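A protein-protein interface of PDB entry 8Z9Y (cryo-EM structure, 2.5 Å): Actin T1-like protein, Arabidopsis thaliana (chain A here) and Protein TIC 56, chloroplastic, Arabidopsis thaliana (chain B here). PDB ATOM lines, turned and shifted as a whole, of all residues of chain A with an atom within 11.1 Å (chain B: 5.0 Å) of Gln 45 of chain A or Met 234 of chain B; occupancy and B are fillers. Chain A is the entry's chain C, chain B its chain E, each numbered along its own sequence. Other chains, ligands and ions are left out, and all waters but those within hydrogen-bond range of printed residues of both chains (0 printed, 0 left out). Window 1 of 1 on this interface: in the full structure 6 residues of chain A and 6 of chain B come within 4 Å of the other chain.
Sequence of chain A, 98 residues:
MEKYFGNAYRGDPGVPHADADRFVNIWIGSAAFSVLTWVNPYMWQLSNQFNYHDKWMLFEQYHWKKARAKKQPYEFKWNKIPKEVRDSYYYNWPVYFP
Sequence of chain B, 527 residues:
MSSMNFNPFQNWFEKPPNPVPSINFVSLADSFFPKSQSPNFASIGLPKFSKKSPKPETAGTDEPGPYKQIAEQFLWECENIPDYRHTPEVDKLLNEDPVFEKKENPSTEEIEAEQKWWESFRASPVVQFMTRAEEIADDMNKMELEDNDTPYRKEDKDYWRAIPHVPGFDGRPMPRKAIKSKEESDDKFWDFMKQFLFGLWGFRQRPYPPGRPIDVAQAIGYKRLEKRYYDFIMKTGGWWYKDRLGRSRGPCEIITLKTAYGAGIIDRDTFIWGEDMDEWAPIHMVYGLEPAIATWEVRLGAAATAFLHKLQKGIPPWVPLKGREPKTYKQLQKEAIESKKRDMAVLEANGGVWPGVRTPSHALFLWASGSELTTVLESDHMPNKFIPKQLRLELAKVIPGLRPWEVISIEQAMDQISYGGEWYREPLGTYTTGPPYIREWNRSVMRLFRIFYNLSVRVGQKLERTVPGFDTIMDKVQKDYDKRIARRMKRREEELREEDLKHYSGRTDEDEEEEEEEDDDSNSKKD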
ATOM      1  N   THR A  37     -21.064 -14.937   4.221  1.00  0.00           N
ATOM      2  CA  THR A  37     -20.207 -15.714   5.108  1.00  0.00           C
ATOM      3  C   THR A  37     -20.744 -17.129   5.278  1.00  0.00           C
ATOM      4  O   THR A  37     -19.973 -18.094   5.327  1.00  0.00           O
ATOM      5  CB  THR A  37     -20.080 -15.016   6.461  1.00  0.00           C
ATOM      6  OG1 THR A  37     -19.273 -13.841   6.317  1.00  0.00           O
ATOM      7  CG2 THR A  37     -19.425 -15.936   7.472  1.00  0.00           C
ATOM      8  N   VAL A  39     -22.257 -18.691   2.949  1.00  0.00           N
ATOM      9  CA  VAL A  39     -21.877 -19.349   1.702  1.00  0.00           C
ATOM     10  C   VAL A  39     -20.406 -19.753   1.734  1.00  0.00           C
ATOM     11  O   VAL A  39     -20.051 -20.889   1.398  1.00  0.00           O
ATOM     12  CB  VAL A  39     -22.191 -18.439   0.501  1.00  0.00           C
ATOM     13  CG1 VAL A  39     -21.256 -18.738  -0.664  1.00  0.00           C
ATOM     14  CG2 VAL A  39     -23.643 -18.603   0.080  1.00  0.00           C
ATOM     15  N   ASN A  40     -19.530 -18.836   2.144  1.00  0.00           N
ATOM     16  CA  ASN A  40     -18.085 -19.069   2.155  1.00  0.00           C
ATOM     17  C   ASN A  40     -17.523 -18.707   3.524  1.00  0.00           C
ATOM     18  O   ASN A  40     -17.207 -17.540   3.789  1.00  0.00           O
ATOM     19  CB  ASN A  40     -17.391 -18.273   1.053  1.00  0.00           C
ATOM     20  CG  ASN A  40     -15.909 -18.571   0.965  1.00  0.00           C
ATOM     21  OD1 ASN A  40     -15.439 -19.594   1.463  1.00  0.00           O
ATOM     22  ND2 ASN A  40     -15.163 -17.678   0.327  1.00  0.00           N
ATOM     23  N   PRO A  41     -17.387 -19.686   4.422  1.00  0.00           N
ATOM     24  CA  PRO A  41     -16.870 -19.374   5.764  1.00  0.00           C
ATOM     25  C   PRO A  41     -15.407 -18.969   5.778  1.00  0.00           C
ATOM     26  O   PRO A  41     -15.008 -18.175   6.638  1.00  0.00           O
ATOM     27  CB  PRO A  41     -17.097 -20.678   6.546  1.00  0.00           C
ATOM     28  CG  PRO A  41     -17.977 -21.531   5.675  1.00  0.00           C
ATOM     29  CD  PRO A  41     -17.709 -21.112   4.270  1.00  0.00           C
ATOM     30  N   TYR A  42     -14.592 -19.489   4.859  1.00  0.00           N
ATOM     31  CA  TYR A  42     -13.147 -19.254   4.877  1.00  0.00           C
ATOM     32  C   TYR A  42     -12.838 -17.900   4.234  1.00  0.00           C
ATOM     33  O   TYR A  42     -12.307 -17.797   3.127  1.00  0.00           O
ATOM     34  CB  TYR A  42     -12.414 -20.388   4.174  1.00  0.00           C
ATOM     35  CG  TYR A  42     -13.019 -21.750   4.419  1.00  0.00           C
ATOM     36  CD1 TYR A  42     -12.722 -22.466   5.570  1.00  0.00           C
ATOM     37  CD2 TYR A  42     -13.885 -22.322   3.497  1.00  0.00           C
ATOM     38  CE1 TYR A  42     -13.271 -23.711   5.798  1.00  0.00           C
ATOM     39  CE2 TYR A  42     -14.440 -23.565   3.717  1.00  0.00           C
ATOM     40  CZ  TYR A  42     -14.131 -24.256   4.868  1.00  0.00           C
ATOM     41  OH  TYR A  42     -14.682 -25.496   5.089  1.00  0.00           O
ATOM     42  N   MET A  43     -13.185 -16.841   4.964  1.00  0.00           N
ATOM     43  CA  MET A  43     -12.940 -15.488   4.482  1.00  0.00           C
ATOM     44  C   MET A  43     -11.491 -15.054   4.652  1.00  0.00           C
ATOM     45  O   MET A  43     -11.076 -14.074   4.025  1.00  0.00           O
ATOM     46  CB  MET A  43     -13.867 -14.499   5.193  1.00  0.00           C
ATOM     47  CG  MET A  43     -13.298 -13.903   6.466  1.00  0.00           C
ATOM     48  SD  MET A  43     -14.503 -12.870   7.318  1.00  0.00           S
ATOM     49  CE  MET A  43     -13.595 -12.443   8.797  1.00  0.00           C
ATOM     50  N   TRP A  44     -10.714 -15.748   5.484  1.00  0.00           N
ATOM     51  CA  TRP A  44      -9.298 -15.435   5.615  1.00  0.00           C
ATOM     52  C   TRP A  44      -8.472 -15.950   4.444  1.00  0.00           C
ATOM     53  O   TRP A  44      -7.320 -15.530   4.288  1.00  0.00           O
ATOM     54  CB  TRP A  44      -8.744 -16.008   6.922  1.00  0.00           C
ATOM     55  CG  TRP A  44      -8.854 -17.496   7.023  1.00  0.00           C
ATOM     56  CD1 TRP A  44      -7.991 -18.419   6.509  1.00  0.00           C
ATOM     57  CD2 TRP A  44      -9.889 -18.236   7.680  1.00  0.00           C
ATOM     58  NE1 TRP A  44      -8.424 -19.688   6.804  1.00  0.00           N
ATOM     59  CE2 TRP A  44      -9.588 -19.603   7.523  1.00  0.00           C
ATOM     60  CE3 TRP A  44     -11.040 -17.877   8.385  1.00  0.00           C
ATOM     61  CZ2 TRP A  44     -10.396 -20.610   8.045  1.00  0.00           C
ATOM     62  CZ3 TRP A  44     -11.841 -18.877   8.902  1.00  0.00           C
ATOM     63  CH2 TRP A  44     -11.515 -20.226   8.730  1.00  0.00           C
ATOM     64  N   GLN A  45      -9.027 -16.844   3.624  1.00  0.00           N
ATOM     65  CA  GLN A  45      -8.294 -17.390   2.489  1.00  0.00           C
ATOM     66  C   GLN A  45      -8.158 -16.403   1.340  1.00  0.00           C
ATOM     67  O   GLN A  45      -7.382 -16.667   0.415  1.00  0.00           O
ATOM     68  CB  GLN A  45      -8.971 -18.668   1.992  1.00  0.00           C
ATOM     69  CG  GLN A  45      -8.788 -19.865   2.908  1.00  0.00           C
ATOM     70  CD  GLN A  45      -7.435 -20.531   2.742  1.00  0.00           C
ATOM     71  OE1 GLN A  45      -6.597 -20.079   1.962  1.00  0.00           O
ATOM     72  NE2 GLN A  45      -7.216 -21.614   3.479  1.00  0.00           N
ATOM     73  N   LEU A  46      -8.892 -15.293   1.362  1.00  0.00           N
ATOM     74  CA  LEU A  46      -8.724 -14.271   0.338  1.00  0.00           C
ATOM     75  C   LEU A  46      -7.305 -13.719   0.388  1.00  0.00           C
ATOM     76  O   LEU A  46      -6.781 -13.414   1.462  1.00  0.00           O
ATOM     77  CB  LEU A  46      -9.743 -13.143   0.522  1.00  0.00           C
ATOM     78  CG  LEU A  46     -11.220 -13.362   0.160  1.00  0.00           C
ATOM     79  CD1 LEU A  46     -11.366 -13.609  -1.335  1.00  0.00           C
ATOM     80  CD2 LEU A  46     -11.892 -14.469   0.962  1.00  0.00           C
ATOM     81  N   SER A  47      -6.685 -13.594  -0.781  1.00  0.00           N
ATOM     82  CA  SER A  47      -5.285 -13.222  -0.889  1.00  0.00           C
ATOM     83  C   SER A  47      -5.138 -11.936  -1.689  1.00  0.00           C
ATOM     84  O   SER A  47      -5.947 -11.639  -2.573  1.00  0.00           O
ATOM     85  CB  SER A  47      -4.467 -14.336  -1.550  1.00  0.00           C
ATOM     86  OG  SER A  47      -5.183 -14.920  -2.624  1.00  0.00           O
ATOM     87  N   ASN A  48      -4.094 -11.179  -1.370  1.00  0.00           N
ATOM     88  CA  ASN A  48      -3.821  -9.939  -2.075  1.00  0.00           C
ATOM     89  C   ASN A  48      -3.338 -10.225  -3.495  1.00  0.00           C
ATOM     90  O   ASN A  48      -2.976 -11.352  -3.845  1.00  0.00           O
ATOM     91  CB  ASN A  48      -2.780  -9.113  -1.323  1.00  0.00           C
ATOM     92  CG  ASN A  48      -3.244  -8.717   0.062  1.00  0.00           C
ATOM     93  OD1 ASN A  48      -4.414  -8.398   0.269  1.00  0.00           O
ATOM     94  ND2 ASN A  48      -2.328  -8.738   1.022  1.00  0.00           N
ATOM     95  N   GLN A  49      -3.342  -9.177  -4.320  1.00  0.00           N
ATOM     96  CA  GLN A  49      -2.952  -9.333  -5.717  1.00  0.00           C
ATOM     97  C   GLN A  49      -1.468  -9.658  -5.849  1.00  0.00           C
ATOM     98  O   GLN A  49      -1.079 -10.470  -6.696  1.00  0.00           O
ATOM     99  CB  GLN A  49      -3.309  -8.069  -6.498  1.00  0.00           C
ATOM    100  CG  GLN A  49      -2.414  -7.787  -7.690  1.00  0.00           C
ATOM    101  CD  GLN A  49      -3.093  -6.921  -8.731  1.00  0.00           C
ATOM    102  OE1 GLN A  49      -4.285  -6.632  -8.631  1.00  0.00           O
ATOM    103  NE2 GLN A  49      -2.336  -6.500  -9.736  1.00  0.00           N
ATOM    104  N   TRP A  93       4.328 -12.940   7.667  1.00  0.00           N
ATOM    105  CA  TRP A  93       3.771 -13.084   6.325  1.00  0.00           C
ATOM    106  C   TRP A  93       2.750 -14.212   6.182  1.00  0.00           C
ATOM    107  O   TRP A  93       1.730 -13.984   5.509  1.00  0.00           O
ATOM    108  CB  TRP A  93       4.909 -13.224   5.300  1.00  0.00           C
ATOM    109  CG  TRP A  93       5.433 -14.608   5.092  1.00  0.00           C
ATOM    110  CD1 TRP A  93       6.510 -15.178   5.706  1.00  0.00           C
ATOM    111  CD2 TRP A  93       4.911 -15.597   4.198  1.00  0.00           C
ATOM    112  NE1 TRP A  93       6.685 -16.464   5.254  1.00  0.00           N
ATOM    113  CE2 TRP A  93       5.717 -16.745   4.327  1.00  0.00           C
ATOM    114  CE3 TRP A  93       3.837 -15.624   3.303  1.00  0.00           C
ATOM    115  CZ2 TRP A  93       5.483 -17.906   3.595  1.00  0.00           C
ATOM    116  CZ3 TRP A  93       3.607 -16.779   2.579  1.00  0.00           C
ATOM    117  CH2 TRP A  93       4.426 -17.903   2.729  1.00  0.00           C
ATOM    118  N   PRO A  94       2.930 -15.413   6.751  1.00  0.00           N
ATOM    119  CA  PRO A  94       1.957 -16.483   6.465  1.00  0.00           C
ATOM    120  C   PRO A  94       0.541 -16.154   6.899  1.00  0.00           C
ATOM    121  O   PRO A  94      -0.414 -16.657   6.293  1.00  0.00           O
ATOM    122  CB  PRO A  94       2.514 -17.687   7.241  1.00  0.00           C
ATOM    123  CG  PRO A  94       3.926 -17.345   7.536  1.00  0.00           C
ATOM    124  CD  PRO A  94       3.931 -15.873   7.730  1.00  0.00           C
ATOM    125  N   VAL A  95       0.371 -15.325   7.924  1.00  0.00           N
ATOM    126  CA  VAL A  95      -0.948 -14.990   8.442  1.00  0.00           C
ATOM    127  C   VAL A  95      -1.431 -13.634   7.937  1.00  0.00           C
ATOM    128  O   VAL A  95      -2.611 -13.472   7.626  1.00  0.00           O
ATOM    129  CB  VAL A  95      -0.941 -15.050   9.985  1.00  0.00           C
ATOM    130  CG1 VAL A  95       0.193 -14.214  10.553  1.00  0.00           C
ATOM    131  CG2 VAL A  95      -2.280 -14.595  10.547  1.00  0.00           C
ATOM    132  N   TYR A  96      -0.537 -12.651   7.832  1.00  0.00           N
ATOM    133  CA  TYR A  96      -0.952 -11.302   7.463  1.00  0.00           C
ATOM    134  C   TYR A  96      -0.862 -11.039   5.965  1.00  0.00           C
ATOM    135  O   TYR A  96      -1.769 -10.425   5.393  1.00  0.00           O
ATOM    136  CB  TYR A  96      -0.118 -10.267   8.221  1.00  0.00           C
ATOM    137  CG  TYR A  96      -0.526 -10.103   9.666  1.00  0.00           C
ATOM    138  CD1 TYR A  96      -1.629  -9.336  10.011  1.00  0.00           C
ATOM    139  CD2 TYR A  96       0.192 -10.711  10.685  1.00  0.00           C
ATOM    140  CE1 TYR A  96      -2.008  -9.184  11.328  1.00  0.00           C
ATOM    141  CE2 TYR A  96      -0.179 -10.563  12.007  1.00  0.00           C
ATOM    142  CZ  TYR A  96      -1.280  -9.798  12.322  1.00  0.00           C
ATOM    143  OH  TYR A  96      -1.656  -9.645  13.637  1.00  0.00           O
ATOM    144  N   PHE A  97       0.208 -11.486   5.311  1.00  0.00           N
ATOM    145  CA  PHE A  97       0.422 -11.249   3.883  1.00  0.00           C
ATOM    146  C   PHE A  97       0.694 -12.579   3.194  1.00  0.00           C
ATOM    147  O   PHE A  97       1.830 -12.870   2.799  1.00  0.00           O
ATOM    148  CB  PHE A  97       1.580 -10.276   3.656  1.00  0.00           C
ATOM    149  CG  PHE A  97       1.768  -9.285   4.766  1.00  0.00           C
ATOM    150  CD1 PHE A  97       0.840  -8.282   4.985  1.00  0.00           C
ATOM    151  CD2 PHE A  97       2.875  -9.358   5.595  1.00  0.00           C
ATOM    152  CE1 PHE A  97       1.015  -7.372   6.009  1.00  0.00           C
ATOM    153  CE2 PHE A  97       3.054  -8.451   6.619  1.00  0.00           C
ATOM    154  CZ  PHE A  97       2.124  -7.456   6.826  1.00  0.00           C
ATOM    155  N   PRO A  98      -0.337 -13.424   3.035  1.00  0.00           N
ATOM    156  CA  PRO A  98      -0.159 -14.762   2.459  1.00  0.00           C
ATOM    157  C   PRO A  98       0.327 -14.722   1.014  1.00  0.00           C
ATOM    158  O   PRO A  98       0.109 -13.745   0.298  1.00  0.00           O
ATOM    159  CB  PRO A  98      -1.564 -15.373   2.539  1.00  0.00           C
ATOM    160  CG  PRO A  98      -2.309 -14.529   3.522  1.00  0.00           C
ATOM    161  CD  PRO A  98      -1.743 -13.158   3.376  1.00  0.00           C
ATOM    162  OXT PRO A  98       0.951 -15.666   0.530  1.00  0.00           O
ATOM    163  N   TYR B 229     -12.128 -33.526   6.019  1.00  0.00           N
ATOM    164  CA  TYR B 229     -10.733 -33.150   5.869  1.00  0.00           C
ATOM    165  C   TYR B 229     -10.522 -32.074   4.815  1.00  0.00           C
ATOM    166  O   TYR B 229      -9.486 -31.411   4.843  1.00  0.00           O
ATOM    167  CB  TYR B 229      -9.886 -34.386   5.581  1.00  0.00           C
ATOM    168  CG  TYR B 229      -9.494 -35.079   6.863  1.00  0.00           C
ATOM    169  CD1 TYR B 229      -8.574 -34.502   7.727  1.00  0.00           C
ATOM    170  CD2 TYR B 229     -10.070 -36.285   7.231  1.00  0.00           C
ATOM    171  CE1 TYR B 229      -8.224 -35.116   8.910  1.00  0.00           C
ATOM    172  CE2 TYR B 229      -9.724 -36.908   8.411  1.00  0.00           C
ATOM    173  CZ  TYR B 229      -8.799 -36.320   9.246  1.00  0.00           C
ATOM    174  OH  TYR B 229      -8.449 -36.936  10.425  1.00  0.00           O
ATOM    175  N   TYR B 230     -11.492 -31.836   3.931  1.00  0.00           N
ATOM    176  CA  TYR B 230     -11.475 -30.603   3.152  1.00  0.00           C
ATOM    177  C   TYR B 230     -11.597 -29.396   4.069  1.00  0.00           C
ATOM    178  O   TYR B 230     -10.843 -28.419   3.945  1.00  0.00           O
ATOM    179  CB  TYR B 230     -12.608 -30.621   2.129  1.00  0.00           C
ATOM    180  CG  TYR B 230     -12.899 -29.279   1.500  1.00  0.00           C
ATOM    181  CD1 TYR B 230     -12.072 -28.756   0.517  1.00  0.00           C
ATOM    182  CD2 TYR B 230     -14.007 -28.539   1.885  1.00  0.00           C
ATOM    183  CE1 TYR B 230     -12.339 -27.531  -0.060  1.00  0.00           C
ATOM    184  CE2 TYR B 230     -14.281 -27.315   1.315  1.00  0.00           C
ATOM    185  CZ  TYR B 230     -13.444 -26.816   0.342  1.00  0.00           C
ATOM    186  OH  TYR B 230     -13.717 -25.595  -0.227  1.00  0.00           O
ATOM    187  N   ASP B 231     -12.536 -29.458   5.015  1.00  0.00           N
ATOM    188  CA  ASP B 231     -12.667 -28.376   5.984  1.00  0.00           C
ATOM    189  C   ASP B 231     -11.394 -28.235   6.810  1.00  0.00           C
ATOM    190  O   ASP B 231     -10.944 -27.118   7.089  1.00  0.00           O
ATOM    191  CB  ASP B 231     -13.896 -28.623   6.867  1.00  0.00           C
ATOM    192  CG  ASP B 231     -14.002 -27.664   8.048  1.00  0.00           C
ATOM    193  OD1 ASP B 231     -15.082 -27.054   8.187  1.00  0.00           O
ATOM    194  OD2 ASP B 231     -13.071 -27.558   8.874  1.00  0.00           O
ATOM    195  N   PHE B 232     -10.801 -29.363   7.208  1.00  0.00           N
ATOM    196  CA  PHE B 232      -9.558 -29.326   7.976  1.00  0.00           C
ATOM    197  C   PHE B 232      -8.424 -28.693   7.177  1.00  0.00           C
ATOM    198  O   PHE B 232      -7.657 -27.883   7.709  1.00  0.00           O
ATOM    199  CB  PHE B 232      -9.184 -30.742   8.420  1.00  0.00           C
ATOM    200  CG  PHE B 232      -7.918 -30.821   9.231  1.00  0.00           C
ATOM    201  CD1 PHE B 232      -6.684 -30.958   8.615  1.00  0.00           C
ATOM    202  CD2 PHE B 232      -7.962 -30.764  10.614  1.00  0.00           C
ATOM    203  CE1 PHE B 232      -5.524 -31.032   9.361  1.00  0.00           C
ATOM    204  CE2 PHE B 232      -6.804 -30.837  11.363  1.00  0.00           C
ATOM    205  CZ  PHE B 232      -5.585 -30.971  10.736  1.00  0.00           C
ATOM    206  N   ILE B 233      -8.296 -29.059   5.901  1.00  0.00           N
ATOM    207  CA  ILE B 233      -7.206 -28.558   5.072  1.00  0.00           C
ATOM    208  C   ILE B 233      -7.368 -27.067   4.813  1.00  0.00           C
ATOM    209  O   ILE B 233      -6.381 -26.323   4.748  1.00  0.00           O
ATOM    210  CB  ILE B 233      -7.131 -29.365   3.762  1.00  0.00           C
ATOM    211  CG1 ILE B 233      -6.426 -30.700   4.001  1.00  0.00           C
ATOM    212  CG2 ILE B 233      -6.424 -28.581   2.669  1.00  0.00           C
ATOM    213  CD1 ILE B 233      -6.442 -31.615   2.801  1.00  0.00           C
ATOM    214  N   MET B 234      -8.610 -26.600   4.675  1.00  0.00           N
ATOM    215  CA  MET B 234      -8.825 -25.190   4.371  1.00  0.00           C
ATOM    216  C   MET B 234      -8.326 -24.262   5.476  1.00  0.00           C
ATOM    217  O   MET B 234      -8.167 -23.062   5.230  1.00  0.00           O
ATOM    218  CB  MET B 234     -10.307 -24.930   4.104  1.00  0.00           C
ATOM    219  CG  MET B 234     -10.709 -25.116   2.653  1.00  0.00           C
ATOM    220  SD  MET B 234      -9.739 -24.083   1.541  1.00  0.00           S
ATOM    221  CE  MET B 234     -10.916 -23.812   0.220  1.00  0.00           C
ATOM    222  N   LYS B 235      -8.073 -24.780   6.679  1.00  0.00           N
ATOM    223  CA  LYS B 235      -7.633 -23.963   7.805  1.00  0.00           C
ATOM    224  C   LYS B 235      -6.181 -24.224   8.199  1.00  0.00           C
ATOM    225  O   LYS B 235      -5.774 -23.854   9.304  1.00  0.00           O
ATOM    226  CB  LYS B 235      -8.537 -24.190   9.017  1.00  0.00           C
ATOM    227  CG  LYS B 235     -10.020 -24.044   8.749  1.00  0.00           C
ATOM    228  CD  LYS B 235     -10.811 -24.273  10.025  1.00  0.00           C
ATOM    229  CE  LYS B 235     -12.306 -24.226   9.772  1.00  0.00           C
ATOM    230  NZ  LYS B 235     -13.074 -24.766  10.926  1.00  0.00           N
ATOM    231  N   THR B 236      -5.391 -24.851   7.333  1.00  0.00           N
ATOM    232  CA  THR B 236      -4.022 -25.209   7.674  1.00  0.00           C
ATOM    233  C   THR B 236      -3.059 -24.690   6.615  1.00  0.00           C
ATOM    234  O   THR B 236      -3.432 -24.447   5.464  1.00  0.00           O
ATOM    235  CB  THR B 236      -3.856 -26.728   7.834  1.00  0.00           C
ATOM    236  OG1 THR B 236      -2.581 -27.010   8.426  1.00  0.00           O
ATOM    237  CG2 THR B 236      -3.944 -27.426   6.494  1.00  0.00           C
ATOM    238  N   ILE B 254      -2.079 -22.393   0.860  1.00  0.00           N
ATOM    239  CA  ILE B 254      -3.018 -22.886  -0.144  1.00  0.00           C
ATOM    240  C   ILE B 254      -2.926 -22.047  -1.412  1.00  0.00           C
ATOM    241  O   ILE B 254      -3.026 -22.569  -2.528  1.00  0.00           O
ATOM    242  CB  ILE B 254      -4.448 -22.910   0.426  1.00  0.00           C
ATOM    243  CG1 ILE B 254      -4.497 -23.777   1.682  1.00  0.00           C
ATOM    244  CG2 ILE B 254      -5.427 -23.433  -0.610  1.00  0.00           C
ATOM    245  CD1 ILE B 254      -4.241 -25.243   1.417  1.00  0.00           C
ATOM    246  N   ALA B 292      -9.608 -28.611  -2.657  1.00  0.00           N
ATOM    247  CA  ALA B 292      -9.132 -27.348  -2.105  1.00  0.00           C
ATOM    248  C   ALA B 292      -8.233 -26.609  -3.089  1.00  0.00           C
ATOM    249  O   ALA B 292      -8.274 -25.377  -3.170  1.00  0.00           O
ATOM    250  CB  ALA B 292      -8.397 -27.596  -0.789  1.00  0.00           C
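The side-chain hydroxyl of Tyr 42 of chain A is in hydrogen-bond range of the side-chain carboxylate of Asp 231 of chain B (3.5 Å).
O of Met 234 of chain B lies within hydrogen-bond range of NE2 of Gln 45 of chain A, at 2.5 Å.
Printed residues of chain B within 4 Å of Tyr 42 of chain A: Asp 231 and Met 234.
Of the printed residues of chain B, Trp 44 of chain A touches Met 234 (3.7 Å) and Lys 235 (3.5 Å).
Gln 45 of chain A touches just these residues of chain B: Met 234 and Ile 254.
Tyr 96 of chain A touches none of the printed residues of chain B.
No residue of chain A comes within 4 Å of Tyr 230 of chain B.
Asp 231 of chain B touches just one residue of chain A: Tyr 42 (3.5 Å).
No residue of chain A comes within 4 Å of Ile 233 of chain B.
Of chain A, only Tyr 42, Trp 44 and Gln 45 come within 4 Å of Met 234 of chain B.
Printed residues of chain A within 4 Å of Lys 235 of chain B: Trp 44.
No residue of chain A comes within 4 Å of Thr 236 of chain B.
The nearest residue of chain A that does not touch Met 234 of chain B is Asn 40 of chain A (6.3 Å).
The nearest printed residue of chain B that does not touch Tyr 42 of chain A is Lys 235 of chain B (4.1 Å).
Of the 10 printed residues of chain B, 4 touch a printed residue of chain A.
Hydrophobic or aromatic side chains of chain B within 4 Å of the printed part of chain A: Met 234 and Ile 254.
Along chain B the printed residues that touch a printed residue of chain A span positions 231 to 254.
Of the 18 printed residues of chain A, 3 touch a printed residue of chain B.
Hydrophobic or aromatic side chains of chain A within 4 Å of the printed part of chain B: Tyr 42 and Trp 44.
Among the printed residues, 6 pairs touch across the chains.
Among the printed residues, no Asp or Glu carboxylate lies within 4 Å of a Lys or Arg side-chain nitrogen of the other chain.
NZ of Lys 235 of chain B lies within salt-bridge range of OD2 of Asp 231 of chain B, at 3.5 Å.
Among the printed residues, pairs that only touch across the chains: Tyr 42 of chain A with Met 234 of chain B (3.6 Å), Trp 44 of chain A with Met 234 of chain B (3.7 Å), Trp 44 of chain A with Lys 235 of chain B (3.5 Å) and Gln 45 of chain A with Ile 254 of chain B (3.9 Å).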
